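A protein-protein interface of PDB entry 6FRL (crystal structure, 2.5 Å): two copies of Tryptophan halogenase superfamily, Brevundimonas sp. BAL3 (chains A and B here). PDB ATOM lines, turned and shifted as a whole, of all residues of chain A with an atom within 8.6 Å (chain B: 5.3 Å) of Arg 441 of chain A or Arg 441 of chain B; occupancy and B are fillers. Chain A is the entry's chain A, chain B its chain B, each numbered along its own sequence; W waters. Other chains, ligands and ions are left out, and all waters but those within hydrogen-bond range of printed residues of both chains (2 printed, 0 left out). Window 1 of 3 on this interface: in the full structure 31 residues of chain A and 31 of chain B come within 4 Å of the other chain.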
ATOM      1  N   ARG A 364      12.981  -5.574 -12.832  1.00  0.00           N
ATOM      2  CA  ARG A 364      11.798  -6.271 -12.383  1.00  0.00           C
ATOM      3  C   ARG A 364      10.485  -5.627 -12.912  1.00  0.00           C
ATOM      4  O   ARG A 364       9.562  -6.313 -13.305  1.00  0.00           O
ATOM      5  CB  ARG A 364      11.865  -6.348 -10.850  1.00  0.00           C
ATOM      6  CG  ARG A 364      10.864  -7.239 -10.162  1.00  0.00           C
ATOM      7  CD  ARG A 364      11.142  -7.266  -8.660  1.00  0.00           C
ATOM      8  NE  ARG A 364      12.368  -8.030  -8.375  1.00  0.00           N
ATOM      9  CZ  ARG A 364      13.470  -7.589  -7.772  1.00  0.00           C
ATOM     10  NH1 ARG A 364      13.567  -6.368  -7.295  1.00  0.00           N
ATOM     11  NH2 ARG A 364      14.500  -8.420  -7.633  1.00  0.00           N
ATOM     12  N   GLU A 381       4.102 -11.284  -7.076  1.00  0.00           N
ATOM     13  CA  GLU A 381       5.454 -11.705  -7.460  1.00  0.00           C
ATOM     14  C   GLU A 381       6.481 -10.558  -7.315  1.00  0.00           C
ATOM     15  O   GLU A 381       7.524 -10.765  -6.741  1.00  0.00           O
ATOM     16  CB  GLU A 381       5.456 -12.257  -8.894  1.00  0.00           C
ATOM     17  CG  GLU A 381       6.792 -12.809  -9.395  1.00  0.00           C
ATOM     18  CD  GLU A 381       7.312 -14.021  -8.629  1.00  0.00           C
ATOM     19  OE1 GLU A 381       6.592 -14.654  -7.791  1.00  0.00           O
ATOM     20  OE2 GLU A 381       8.477 -14.367  -8.901  1.00  0.00           O
ATOM     21  N   ASP A 384       7.023  -9.923  -3.651  1.00  0.00           N
ATOM     22  CA  ASP A 384       7.754 -11.050  -3.066  1.00  0.00           C
ATOM     23  C   ASP A 384       9.261 -11.029  -3.436  1.00  0.00           C
ATOM     24  O   ASP A 384      10.122 -11.181  -2.573  1.00  0.00           O
ATOM     25  CB  ASP A 384       7.101 -12.399  -3.439  1.00  0.00           C
ATOM     26  CG  ASP A 384       7.702 -13.558  -2.648  1.00  0.00           C
ATOM     27  OD1 ASP A 384       7.524 -13.598  -1.402  1.00  0.00           O
ATOM     28  OD2 ASP A 384       8.399 -14.415  -3.253  1.00  0.00           O
ATOM     29  N   GLN A 385       9.579 -10.822  -4.702  1.00  0.00           N
ATOM     30  CA  GLN A 385      10.986 -10.748  -5.114  1.00  0.00           C
ATOM     31  C   GLN A 385      11.682  -9.609  -4.361  1.00  0.00           C
ATOM     32  O   GLN A 385      12.733  -9.821  -3.740  1.00  0.00           O
ATOM     33  CB  GLN A 385      11.131 -10.528  -6.636  1.00  0.00           C
ATOM     34  CG  GLN A 385      10.649 -11.676  -7.513  1.00  0.00           C
ATOM     35  CD  GLN A 385      10.859 -11.462  -9.003  1.00  0.00           C
ATOM     36  OE1 GLN A 385      11.663 -10.619  -9.449  1.00  0.00           O
ATOM     37  NE2 GLN A 385      10.128 -12.233  -9.788  1.00  0.00           N
ATOM     38  N   ALA A 387      10.981  -7.927  -1.568  1.00  0.00           N
ATOM     39  CA  ALA A 387      11.129  -8.224  -0.145  1.00  0.00           C
ATOM     40  C   ALA A 387      12.283  -9.161   0.130  1.00  0.00           C
ATOM     41  O   ALA A 387      13.154  -8.827   0.937  1.00  0.00           O
ATOM     42  CB  ALA A 387       9.832  -8.810   0.411  1.00  0.00           C
ATOM     43  N   ARG A 388      12.329 -10.305  -0.559  1.00  0.00           N
ATOM     44  CA  ARG A 388      13.398 -11.280  -0.324  1.00  0.00           C
ATOM     45  C   ARG A 388      14.747 -10.662  -0.646  1.00  0.00           C
ATOM     46  O   ARG A 388      15.696 -10.844   0.098  1.00  0.00           O
ATOM     47  CB  ARG A 388      13.219 -12.600  -1.093  1.00  0.00           C
ATOM     48  CG  ARG A 388      11.884 -13.329  -0.928  1.00  0.00           C
ATOM     49  CD  ARG A 388      11.582 -13.834   0.470  1.00  0.00           C
ATOM     50  NE  ARG A 388      11.165 -12.822   1.468  1.00  0.00           N
ATOM     51  CZ  ARG A 388       9.933 -12.292   1.622  1.00  0.00           C
ATOM     52  NH1 ARG A 388       8.909 -12.595   0.819  1.00  0.00           N
ATOM     53  NH2 ARG A 388       9.718 -11.411   2.606  1.00  0.00           N
ATOM     54  N   GLU A 389      14.835  -9.910  -1.733  1.00  0.00           N
ATOM     55  CA  GLU A 389      16.126  -9.297  -2.156  1.00  0.00           C
ATOM     56  C   GLU A 389      16.657  -8.286  -1.091  1.00  0.00           C
ATOM     57  O   GLU A 389      17.855  -8.274  -0.746  1.00  0.00           O
ATOM     58  CB  GLU A 389      15.996  -8.663  -3.561  1.00  0.00           C
ATOM     59  CG  GLU A 389      17.095  -7.690  -3.995  1.00  0.00           C
ATOM     60  CD  GLU A 389      16.858  -7.172  -5.413  1.00  0.00           C
ATOM     61  OE1 GLU A 389      16.232  -6.080  -5.542  1.00  0.00           O
ATOM     62  OE2 GLU A 389      17.268  -7.855  -6.390  1.00  0.00           O
ATOM     63  N   MET A 390      15.754  -7.482  -0.547  1.00  0.00           N
ATOM     64  CA  MET A 390      16.127  -6.564   0.526  1.00  0.00           C
ATOM     65  C   MET A 390      16.667  -7.326   1.725  1.00  0.00           C
ATOM     66  O   MET A 390      17.690  -6.935   2.297  1.00  0.00           O
ATOM     67  CB  MET A 390      14.954  -5.645   0.923  1.00  0.00           C
ATOM     68  CG  MET A 390      14.658  -4.544  -0.113  1.00  0.00           C
ATOM     69  SD  MET A 390      15.975  -3.284  -0.206  1.00  0.00           S
ATOM     70  CE  MET A 390      15.819  -2.466   1.369  1.00  0.00           C
ATOM     71  N   GLU A 391      16.007  -8.423   2.075  1.00  0.00           N
ATOM     72  CA  GLU A 391      16.424  -9.232   3.211  1.00  0.00           C
ATOM     73  C   GLU A 391      17.804  -9.875   2.958  1.00  0.00           C
ATOM     74  O   GLU A 391      18.648  -9.930   3.873  1.00  0.00           O
ATOM     75  CB  GLU A 391      15.374 -10.328   3.524  1.00  0.00           C
ATOM     76  CG  GLU A 391      14.037  -9.850   4.098  1.00  0.00           C
ATOM     77  CD  GLU A 391      12.954 -10.910   4.057  1.00  0.00           C
ATOM     78  OE1 GLU A 391      13.159 -12.020   3.515  1.00  0.00           O
ATOM     79  OE2 GLU A 391      11.868 -10.617   4.551  1.00  0.00           O
ATOM     80  N   ARG A 392      18.024 -10.348   1.718  1.00  0.00           N
ATOM     81  CA  ARG A 392      19.311 -10.925   1.357  1.00  0.00           C
ATOM     82  C   ARG A 392      20.470  -9.884   1.406  1.00  0.00           C
ATOM     83  O   ARG A 392      21.587 -10.219   1.806  1.00  0.00           O
ATOM     84  CB  ARG A 392      19.240 -11.642   0.028  1.00  0.00           C
ATOM     85  CG  ARG A 392      18.197 -12.741  -0.093  1.00  0.00           C
ATOM     86  CD  ARG A 392      18.550 -13.983   0.671  1.00  0.00           C
ATOM     87  NE  ARG A 392      18.395 -13.813   2.111  1.00  0.00           N
ATOM     88  CZ  ARG A 392      17.228 -13.798   2.767  1.00  0.00           C
ATOM     89  NH1 ARG A 392      16.068 -13.965   2.116  1.00  0.00           N
ATOM     90  NH2 ARG A 392      17.234 -13.599   4.091  1.00  0.00           N
ATOM     91  N   VAL A 393      20.196  -8.622   1.112  1.00  0.00           N
ATOM     92  CA  VAL A 393      21.222  -7.565   1.257  1.00  0.00           C
ATOM     93  C   VAL A 393      21.438  -7.169   2.715  1.00  0.00           C
ATOM     94  O   VAL A 393      22.582  -6.960   3.172  1.00  0.00           O
ATOM     95  CB  VAL A 393      20.877  -6.293   0.415  1.00  0.00           C
ATOM     96  CG1 VAL A 393      21.927  -5.183   0.626  1.00  0.00           C
ATOM     97  CG2 VAL A 393      20.731  -6.623  -1.077  1.00  0.00           C
ATOM     98  N   ARG A 426      21.897 -19.717   9.694  1.00  0.00           N
ATOM     99  CA  ARG A 426      22.075 -20.929   8.893  1.00  0.00           C
ATOM    100  C   ARG A 426      23.293 -20.858   7.984  1.00  0.00           C
ATOM    101  O   ARG A 426      24.014 -21.844   7.859  1.00  0.00           O
ATOM    102  CB  ARG A 426      20.833 -21.223   8.066  1.00  0.00           C
ATOM    103  CG  ARG A 426      19.672 -21.809   8.885  1.00  0.00           C
ATOM    104  CD  ARG A 426      18.457 -21.939   7.991  1.00  0.00           C
ATOM    105  NE  ARG A 426      18.781 -22.743   6.806  1.00  0.00           N
ATOM    106  CZ  ARG A 426      18.072 -22.799   5.670  1.00  0.00           C
ATOM    107  NH1 ARG A 426      16.955 -22.090   5.521  1.00  0.00           N
ATOM    108  NH2 ARG A 426      18.488 -23.586   4.673  1.00  0.00           N
ATOM    109  N   LYS A 427      23.498 -19.702   7.352  1.00  0.00           N
ATOM    110  CA  LYS A 427      24.689 -19.466   6.512  1.00  0.00           C
ATOM    111  C   LYS A 427      25.977 -19.601   7.312  1.00  0.00           C
ATOM    112  O   LYS A 427      26.876 -20.333   6.906  1.00  0.00           O
ATOM    113  CB  LYS A 427      24.675 -18.066   5.866  1.00  0.00           C
ATOM    114  CG  LYS A 427      23.924 -17.988   4.549  1.00  0.00           C
ATOM    115  CD  LYS A 427      23.897 -16.582   3.979  1.00  0.00           C
ATOM    116  CE  LYS A 427      24.089 -16.539   2.469  1.00  0.00           C
ATOM    117  NZ  LYS A 427      22.799 -16.830   1.808  1.00  0.00           N
ATOM    118  N   VAL A 438      24.982 -21.522   1.871  1.00  0.00           N
ATOM    119  CA  VAL A 438      23.532 -21.641   1.764  1.00  0.00           C
ATOM    120  C   VAL A 438      23.100 -20.629   0.694  1.00  0.00           C
ATOM    121  O   VAL A 438      23.515 -19.467   0.712  1.00  0.00           O
ATOM    122  CB  VAL A 438      22.811 -21.378   3.110  1.00  0.00           C
ATOM    123  CG1 VAL A 438      21.311 -21.414   2.938  1.00  0.00           C
ATOM    124  CG2 VAL A 438      23.229 -22.407   4.144  1.00  0.00           C
ATOM    125  N   ARG A 439      22.288 -21.089  -0.242  1.00  0.00           N
ATOM    126  CA  ARG A 439      21.866 -20.242  -1.348  1.00  0.00           C
ATOM    127  C   ARG A 439      20.367 -20.058  -1.313  1.00  0.00           C
ATOM    128  O   ARG A 439      19.609 -21.017  -1.400  1.00  0.00           O
ATOM    129  CB  ARG A 439      22.351 -20.809  -2.686  1.00  0.00           C
ATOM    130  CG  ARG A 439      23.869 -20.694  -2.883  1.00  0.00           C
ATOM    131  CD  ARG A 439      24.297 -20.862  -4.344  1.00  0.00           C
ATOM    132  NE  ARG A 439      25.601 -21.525  -4.464  1.00  0.00           N
ATOM    133  CZ  ARG A 439      26.399 -21.499  -5.538  1.00  0.00           C
ATOM    134  NH1 ARG A 439      26.058 -20.829  -6.653  1.00  0.00           N
ATOM    135  NH2 ARG A 439      27.574 -22.149  -5.496  1.00  0.00           N
ATOM    136  N   TYR A 440      19.947 -18.816  -1.110  1.00  0.00           N
ATOM    137  CA  TYR A 440      18.544 -18.455  -1.195  1.00  0.00           C
ATOM    138  C   TYR A 440      18.299 -17.796  -2.560  1.00  0.00           C
ATOM    139  O   TYR A 440      19.236 -17.545  -3.344  1.00  0.00           O
ATOM    140  CB  TYR A 440      18.183 -17.523  -0.044  1.00  0.00           C
ATOM    141  CG  TYR A 440      18.442 -18.075   1.348  1.00  0.00           C
ATOM    142  CD1 TYR A 440      17.713 -19.173   1.856  1.00  0.00           C
ATOM    143  CD2 TYR A 440      19.419 -17.500   2.187  1.00  0.00           C
ATOM    144  CE1 TYR A 440      17.965 -19.686   3.135  1.00  0.00           C
ATOM    145  CE2 TYR A 440      19.666 -17.996   3.478  1.00  0.00           C
ATOM    146  CZ  TYR A 440      18.932 -19.073   3.954  1.00  0.00           C
ATOM    147  OH  TYR A 440      19.180 -19.537   5.224  1.00  0.00           O
ATOM    148  N   ARG A 441      17.032 -17.517  -2.848  1.00  0.00           N
ATOM    149  CA  ARG A 441      16.682 -16.782  -4.082  1.00  0.00           C
ATOM    150  C   ARG A 441      17.001 -15.302  -3.865  1.00  0.00           C
ATOM    151  O   ARG A 441      16.927 -14.796  -2.737  1.00  0.00           O
ATOM    152  CB  ARG A 441      15.202 -16.937  -4.457  1.00  0.00           C
ATOM    153  CG  ARG A 441      14.663 -18.361  -4.502  1.00  0.00           C
ATOM    154  CD  ARG A 441      13.137 -18.390  -4.582  1.00  0.00           C
ATOM    155  NE  ARG A 441      12.458 -17.945  -3.350  1.00  0.00           N
ATOM    156  CZ  ARG A 441      11.248 -17.354  -3.306  1.00  0.00           C
ATOM    157  NH1 ARG A 441      10.545 -17.113  -4.429  1.00  0.00           N
ATOM    158  NH2 ARG A 441      10.724 -16.976  -2.123  1.00  0.00           N
ATOM    159  N   TRP A 442      17.366 -14.636  -4.952  1.00  0.00           N
ATOM    160  CA  TRP A 442      17.462 -13.159  -5.025  1.00  0.00           C
ATOM    161  C   TRP A 442      18.673 -12.540  -4.297  1.00  0.00           C
ATOM    162  O   TRP A 442      18.633 -11.374  -3.892  1.00  0.00           O
ATOM    163  CB  TRP A 442      16.119 -12.507  -4.604  1.00  0.00           C
ATOM    164  CG  TRP A 442      14.943 -13.067  -5.380  1.00  0.00           C
ATOM    165  CD1 TRP A 442      13.901 -13.831  -4.903  1.00  0.00           C
ATOM    166  CD2 TRP A 442      14.749 -12.945  -6.783  1.00  0.00           C
ATOM    167  NE1 TRP A 442      13.063 -14.167  -5.935  1.00  0.00           N
ATOM    168  CE2 TRP A 442      13.561 -13.641  -7.100  1.00  0.00           C
ATOM    169  CE3 TRP A 442      15.458 -12.291  -7.805  1.00  0.00           C
ATOM    170  CZ2 TRP A 442      13.070 -13.723  -8.411  1.00  0.00           C
ATOM    171  CZ3 TRP A 442      14.965 -12.348  -9.112  1.00  0.00           C
ATOM    172  CH2 TRP A 442      13.772 -13.063  -9.403  1.00  0.00           C
ATOM    173  N   GLU A 443      19.749 -13.316  -4.184  1.00  0.00           N
ATOM    174  CA  GLU A 443      21.011 -12.850  -3.622  1.00  0.00           C
ATOM    175  C   GLU A 443      21.691 -11.854  -4.581  1.00  0.00           C
ATOM    176  O   GLU A 443      21.926 -12.172  -5.720  1.00  0.00           O
ATOM    177  CB  GLU A 443      22.005 -14.005  -3.405  1.00  0.00           C
ATOM    178  CG  GLU A 443      21.552 -15.121  -2.476  1.00  0.00           C
ATOM    179  CD  GLU A 443      21.874 -14.922  -1.014  1.00  0.00           C
ATOM    180  OE1 GLU A 443      21.622 -15.901  -0.301  1.00  0.00           O
ATOM    181  OE2 GLU A 443      22.362 -13.848  -0.588  1.00  0.00           O
ATOM    182  N   MET A 444      22.019 -10.676  -4.089  1.00  0.00           N
ATOM    183  CA  MET A 444      22.770  -9.707  -4.853  1.00  0.00           C
ATOM    184  C   MET A 444      24.237 -10.085  -4.875  1.00  0.00           C
ATOM    185  O   MET A 444      24.938  -9.835  -5.880  1.00  0.00           O
ATOM    186  CB  MET A 444      22.593  -8.331  -4.226  1.00  0.00           C
ATOM    187  CG  MET A 444      23.213  -7.232  -5.046  1.00  0.00           C
ATOM    188  SD  MET A 444      22.495  -5.665  -4.582  1.00  0.00           S
ATOM    189  CE  MET A 444      20.918  -5.730  -5.400  1.00  0.00           C
ATOM    190  N   ASP B 384      17.024 -30.266   3.662  1.00  0.00           N
ATOM    191  CA  ASP B 384      16.248 -29.153   3.112  1.00  0.00           C
ATOM    192  C   ASP B 384      16.283 -29.105   1.573  1.00  0.00           C
ATOM    193  O   ASP B 384      15.247 -28.984   0.927  1.00  0.00           O
ATOM    194  CB  ASP B 384      16.689 -27.807   3.726  1.00  0.00           C
ATOM    195  CG  ASP B 384      15.717 -26.677   3.379  1.00  0.00           C
ATOM    196  OD1 ASP B 384      14.543 -26.715   3.806  1.00  0.00           O
ATOM    197  OD2 ASP B 384      16.120 -25.768   2.637  1.00  0.00           O
ATOM    198  N   ARG B 388      12.875 -29.860  -0.899  1.00  0.00           N
ATOM    199  CA  ARG B 388      12.393 -28.862  -1.826  1.00  0.00           C
ATOM    200  C   ARG B 388      12.438 -29.399  -3.250  1.00  0.00           C
ATOM    201  O   ARG B 388      11.487 -29.199  -4.014  1.00  0.00           O
ATOM    202  CB  ARG B 388      13.159 -27.512  -1.738  1.00  0.00           C
ATOM    203  CG  ARG B 388      13.227 -26.863  -0.360  1.00  0.00           C
ATOM    204  CD  ARG B 388      11.880 -26.428   0.227  1.00  0.00           C
ATOM    205  NE  ARG B 388      11.028 -27.500   0.788  1.00  0.00           N
ATOM    206  CZ  ARG B 388      11.149 -28.073   2.015  1.00  0.00           C
ATOM    207  NH1 ARG B 388      12.114 -27.758   2.874  1.00  0.00           N
ATOM    208  NH2 ARG B 388      10.268 -28.993   2.403  1.00  0.00           N
ATOM    209  N   ARG B 392       9.436 -29.731  -5.969  1.00  0.00           N
ATOM    210  CA  ARG B 392       9.496 -29.093  -7.289  1.00  0.00           C
ATOM    211  C   ARG B 392       9.243 -30.083  -8.440  1.00  0.00           C
ATOM    212  O   ARG B 392       8.598 -29.733  -9.415  1.00  0.00           O
ATOM    213  CB  ARG B 392      10.797 -28.311  -7.468  1.00  0.00           C
ATOM    214  CG  ARG B 392      11.072 -27.239  -6.420  1.00  0.00           C
ATOM    215  CD  ARG B 392      10.186 -26.037  -6.559  1.00  0.00           C
ATOM    216  NE  ARG B 392       8.813 -26.300  -6.125  1.00  0.00           N
ATOM    217  CZ  ARG B 392       8.408 -26.368  -4.859  1.00  0.00           C
ATOM    218  NH1 ARG B 392       9.263 -26.186  -3.848  1.00  0.00           N
ATOM    219  NH2 ARG B 392       7.123 -26.631  -4.606  1.00  0.00           N
ATOM    220  N   ARG B 426       0.374 -20.627  -7.623  1.00  0.00           N
ATOM    221  CA  ARG B 426       1.074 -19.376  -7.897  1.00  0.00           C
ATOM    222  C   ARG B 426       1.738 -19.350  -9.272  1.00  0.00           C
ATOM    223  O   ARG B 426       1.693 -18.314  -9.940  1.00  0.00           O
ATOM    224  CB  ARG B 426       2.149 -19.107  -6.838  1.00  0.00           C
ATOM    225  CG  ARG B 426       1.606 -18.620  -5.509  1.00  0.00           C
ATOM    226  CD  ARG B 426       2.752 -18.508  -4.533  1.00  0.00           C
ATOM    227  NE  ARG B 426       3.801 -17.625  -5.086  1.00  0.00           N
ATOM    228  CZ  ARG B 426       5.049 -17.522  -4.628  1.00  0.00           C
ATOM    229  NH1 ARG B 426       5.474 -18.253  -3.589  1.00  0.00           N
ATOM    230  NH2 ARG B 426       5.878 -16.668  -5.219  1.00  0.00           N
ATOM    231  N   ARG B 439      10.018 -18.743 -10.006  1.00  0.00           N
ATOM    232  CA  ARG B 439      11.214 -19.555  -9.860  1.00  0.00           C
ATOM    233  C   ARG B 439      11.476 -19.802  -8.380  1.00  0.00           C
ATOM    234  O   ARG B 439      11.672 -18.868  -7.591  1.00  0.00           O
ATOM    235  CB  ARG B 439      12.398 -18.876 -10.552  1.00  0.00           C
ATOM    236  CG  ARG B 439      12.307 -18.979 -12.082  1.00  0.00           C
ATOM    237  CD  ARG B 439      13.488 -18.339 -12.826  1.00  0.00           C
ATOM    238  NE  ARG B 439      13.041 -17.712 -14.085  1.00  0.00           N
ATOM    239  CZ  ARG B 439      13.782 -17.526 -15.186  1.00  0.00           C
ATOM    240  NH1 ARG B 439      15.061 -17.907 -15.238  1.00  0.00           N
ATOM    241  NH2 ARG B 439      13.228 -16.954 -16.259  1.00  0.00           N
ATOM    242  N   TYR B 440      11.422 -21.069  -8.005  1.00  0.00           N
ATOM    243  CA  TYR B 440      11.807 -21.493  -6.679  1.00  0.00           C
ATOM    244  C   TYR B 440      13.221 -22.074  -6.741  1.00  0.00           C
ATOM    245  O   TYR B 440      13.816 -22.231  -7.821  1.00  0.00           O
ATOM    246  CB  TYR B 440      10.794 -22.505  -6.160  1.00  0.00           C
ATOM    247  CG  TYR B 440       9.342 -22.017  -6.106  1.00  0.00           C
ATOM    248  CD1 TYR B 440       8.945 -20.992  -5.237  1.00  0.00           C
ATOM    249  CD2 TYR B 440       8.354 -22.592  -6.920  1.00  0.00           C
ATOM    250  CE1 TYR B 440       7.618 -20.551  -5.185  1.00  0.00           C
ATOM    251  CE2 TYR B 440       7.014 -22.174  -6.857  1.00  0.00           C
ATOM    252  CZ  TYR B 440       6.656 -21.149  -5.983  1.00  0.00           C
ATOM    253  OH  TYR B 440       5.343 -20.728  -5.942  1.00  0.00           O
ATOM    254  N   ARG B 441      13.784 -22.382  -5.585  1.00  0.00           N
ATOM    255  CA  ARG B 441      15.113 -23.033  -5.529  1.00  0.00           C
ATOM    256  C   ARG B 441      14.907 -24.513  -5.857  1.00  0.00           C
ATOM    257  O   ARG B 441      13.829 -25.096  -5.562  1.00  0.00           O
ATOM    258  CB  ARG B 441      15.784 -22.907  -4.145  1.00  0.00           C
ATOM    259  CG  ARG B 441      15.849 -21.500  -3.563  1.00  0.00           C
ATOM    260  CD  ARG B 441      16.233 -21.500  -2.080  1.00  0.00           C
ATOM    261  NE  ARG B 441      15.206 -22.065  -1.176  1.00  0.00           N
ATOM    262  CZ  ARG B 441      15.450 -22.724  -0.026  1.00  0.00           C
ATOM    263  NH1 ARG B 441      16.695 -22.936   0.406  1.00  0.00           N
ATOM    264  NH2 ARG B 441      14.435 -23.190   0.704  1.00  0.00           N
ATOM    265  N   TRP B 442      15.930 -25.099  -6.472  1.00  0.00           N
ATOM    266  CA  TRP B 442      16.053 -26.564  -6.638  1.00  0.00           C
ATOM    267  C   TRP B 442      15.120 -27.189  -7.686  1.00  0.00           C
ATOM    268  O   TRP B 442      14.787 -28.376  -7.607  1.00  0.00           O
ATOM    269  CB  TRP B 442      15.958 -27.281  -5.265  1.00  0.00           C
ATOM    270  CG  TRP B 442      16.941 -26.715  -4.270  1.00  0.00           C
ATOM    271  CD1 TRP B 442      16.668 -26.015  -3.119  1.00  0.00           C
ATOM    272  CD2 TRP B 442      18.356 -26.780  -4.375  1.00  0.00           C
ATOM    273  NE1 TRP B 442      17.843 -25.666  -2.491  1.00  0.00           N
ATOM    274  CE2 TRP B 442      18.893 -26.114  -3.246  1.00  0.00           C
ATOM    275  CE3 TRP B 442      19.236 -27.355  -5.316  1.00  0.00           C
ATOM    276  CZ2 TRP B 442      20.263 -25.985  -3.040  1.00  0.00           C
ATOM    277  CZ3 TRP B 442      20.610 -27.246  -5.110  1.00  0.00           C
ATOM    278  CH2 TRP B 442      21.112 -26.565  -3.977  1.00  0.00           C
ATOM    279  N   GLU B 443      14.743 -26.396  -8.688  1.00  0.00           N
ATOM    280  CA  GLU B 443      13.943 -26.864  -9.819  1.00  0.00           C
ATOM    281  C   GLU B 443      14.806 -27.780 -10.702  1.00  0.00           C
ATOM    282  O   GLU B 443      15.870 -27.389 -11.152  1.00  0.00           O
ATOM    283  CB  GLU B 443      13.499 -25.684 -10.705  1.00  0.00           C
ATOM    284  CG  GLU B 443      12.649 -24.594 -10.063  1.00  0.00           C
ATOM    285  CD  GLU B 443      11.143 -24.844 -10.094  1.00  0.00           C
ATOM    286  OE1 GLU B 443      10.437 -23.922  -9.681  1.00  0.00           O
ATOM    287  OE2 GLU B 443      10.655 -25.920 -10.512  1.00  0.00           O
HETATM  288  O   HOH W   1      10.092 -16.227  -9.262  1.00  0.00           O
HETATM  289  O   HOH W   2       4.243 -15.230  -7.103  1.00  0.00           O
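NH2 of Arg 426 of chain B is in salt-bridge range of OE1 of Glu 381 of chain A (3.3 Å). The side-chain carboxylate (OD2) of Asp 384 of chain A is in salt-bridge range of the guanidinium group (NH2) of Arg 426 of chain B, 3.9 Å away. The guanidinium group (NH2) of Arg 426 of chain A lies within salt-bridge range of the side-chain carboxylate (OD2) of Asp 384 of chain B, at 3.8 Å.
OE2 of Glu 381 of chain A sits at hydrogen-bond distance from NE2 of Gln 385 of chain A (2.8 Å). The side-chain hydroxyl (OH) of Tyr 440 of chain A lies within hydrogen-bond range of the guanidinium group (NH1) of Arg 426 of chain A, 3.4 Å away. N of Tyr 440 of chain A lies within hydrogen-bond range of OE1 of Glu 443 of chain A, at 3.5 Å. OD1 of Asp 384 of chain B lies within salt-bridge range of NH1 of Arg 388 of chain B, 2.8 Å away. The guanidinium group of Arg 426 of chain B is in hydrogen-bond range of the side-chain hydroxyl of Tyr 440 of chain B, at 3.4 Å. The side-chain carboxylate (OE1) of Glu 443 of chain B lies within hydrogen-bond range of the backbone NH (N) of Tyr 440 of chain B (3.5 Å).
Among the printed residues, pairs that only touch across the chains: Arg 439 of chain A with Arg 441 of chain B, Tyr 440 of chain A with Arg 441 of chain B, Arg 441 of chain A with Arg 439 of chain B, Arg 441 of chain A with Tyr 440 of chain B and Arg 441 of chain A with Arg 441 of chain B.
Of chain B, only Arg 439, Tyr 440 and Arg 441 come within 4 Å of Arg 441 of chain A. Printed residues of chain B within 4 Å of Tyr 440 of chain A: Arg 441 (3.9 Å). Printed residues of chain A within 4 Å of Arg 439 of chain B: Arg 441. Printed residues of chain B within 4 Å of Arg 439 of chain A: Arg 441 (3.5 Å). Arg 388 of chain A touches none of the printed residues of chain B. Arg 392 of chain A touches none of the printed residues of chain B.
Of the 9 printed residues of chain B, 5 touch a printed residue of chain A. Printed residues of chain B that touch a printed residue of chain A: Asp 384, Arg 426, Arg 439, Tyr 440 and Arg 441. Along chain A the printed residues that touch a printed residue of chain B span positions 381 to 441.
Asp 384 of chain A touches Arg 426 of chain B, and with the chains exchanged Arg 426 of chain A touches Asp 384 of chain B. Arg 439 of chain A touches Arg 441 of chain B, and with the chains exchanged Arg 441 of chain A touches Arg 439 of chain B. Tyr 440 of chain A touches Arg 441 of chain B, and with the chains exchanged Arg 441 of chain A touches Tyr 440 of chain B. Arg 441 of chain A touches its own counterpart, Arg 441 of chain B. Positions printed for both chains: 384, 388, 392, 426, 439, 440, 441, 442 and 443.
Water W1 lies within hydrogen-bond range of OE2 of Glu 381 of chain A and N of Arg 439 of chain B. Water W2 bridges the side-chain carboxylate of Glu 381 of chain A (2.5 Å) and the guanidinium group of Arg 426 of chain B (2.9 Å).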
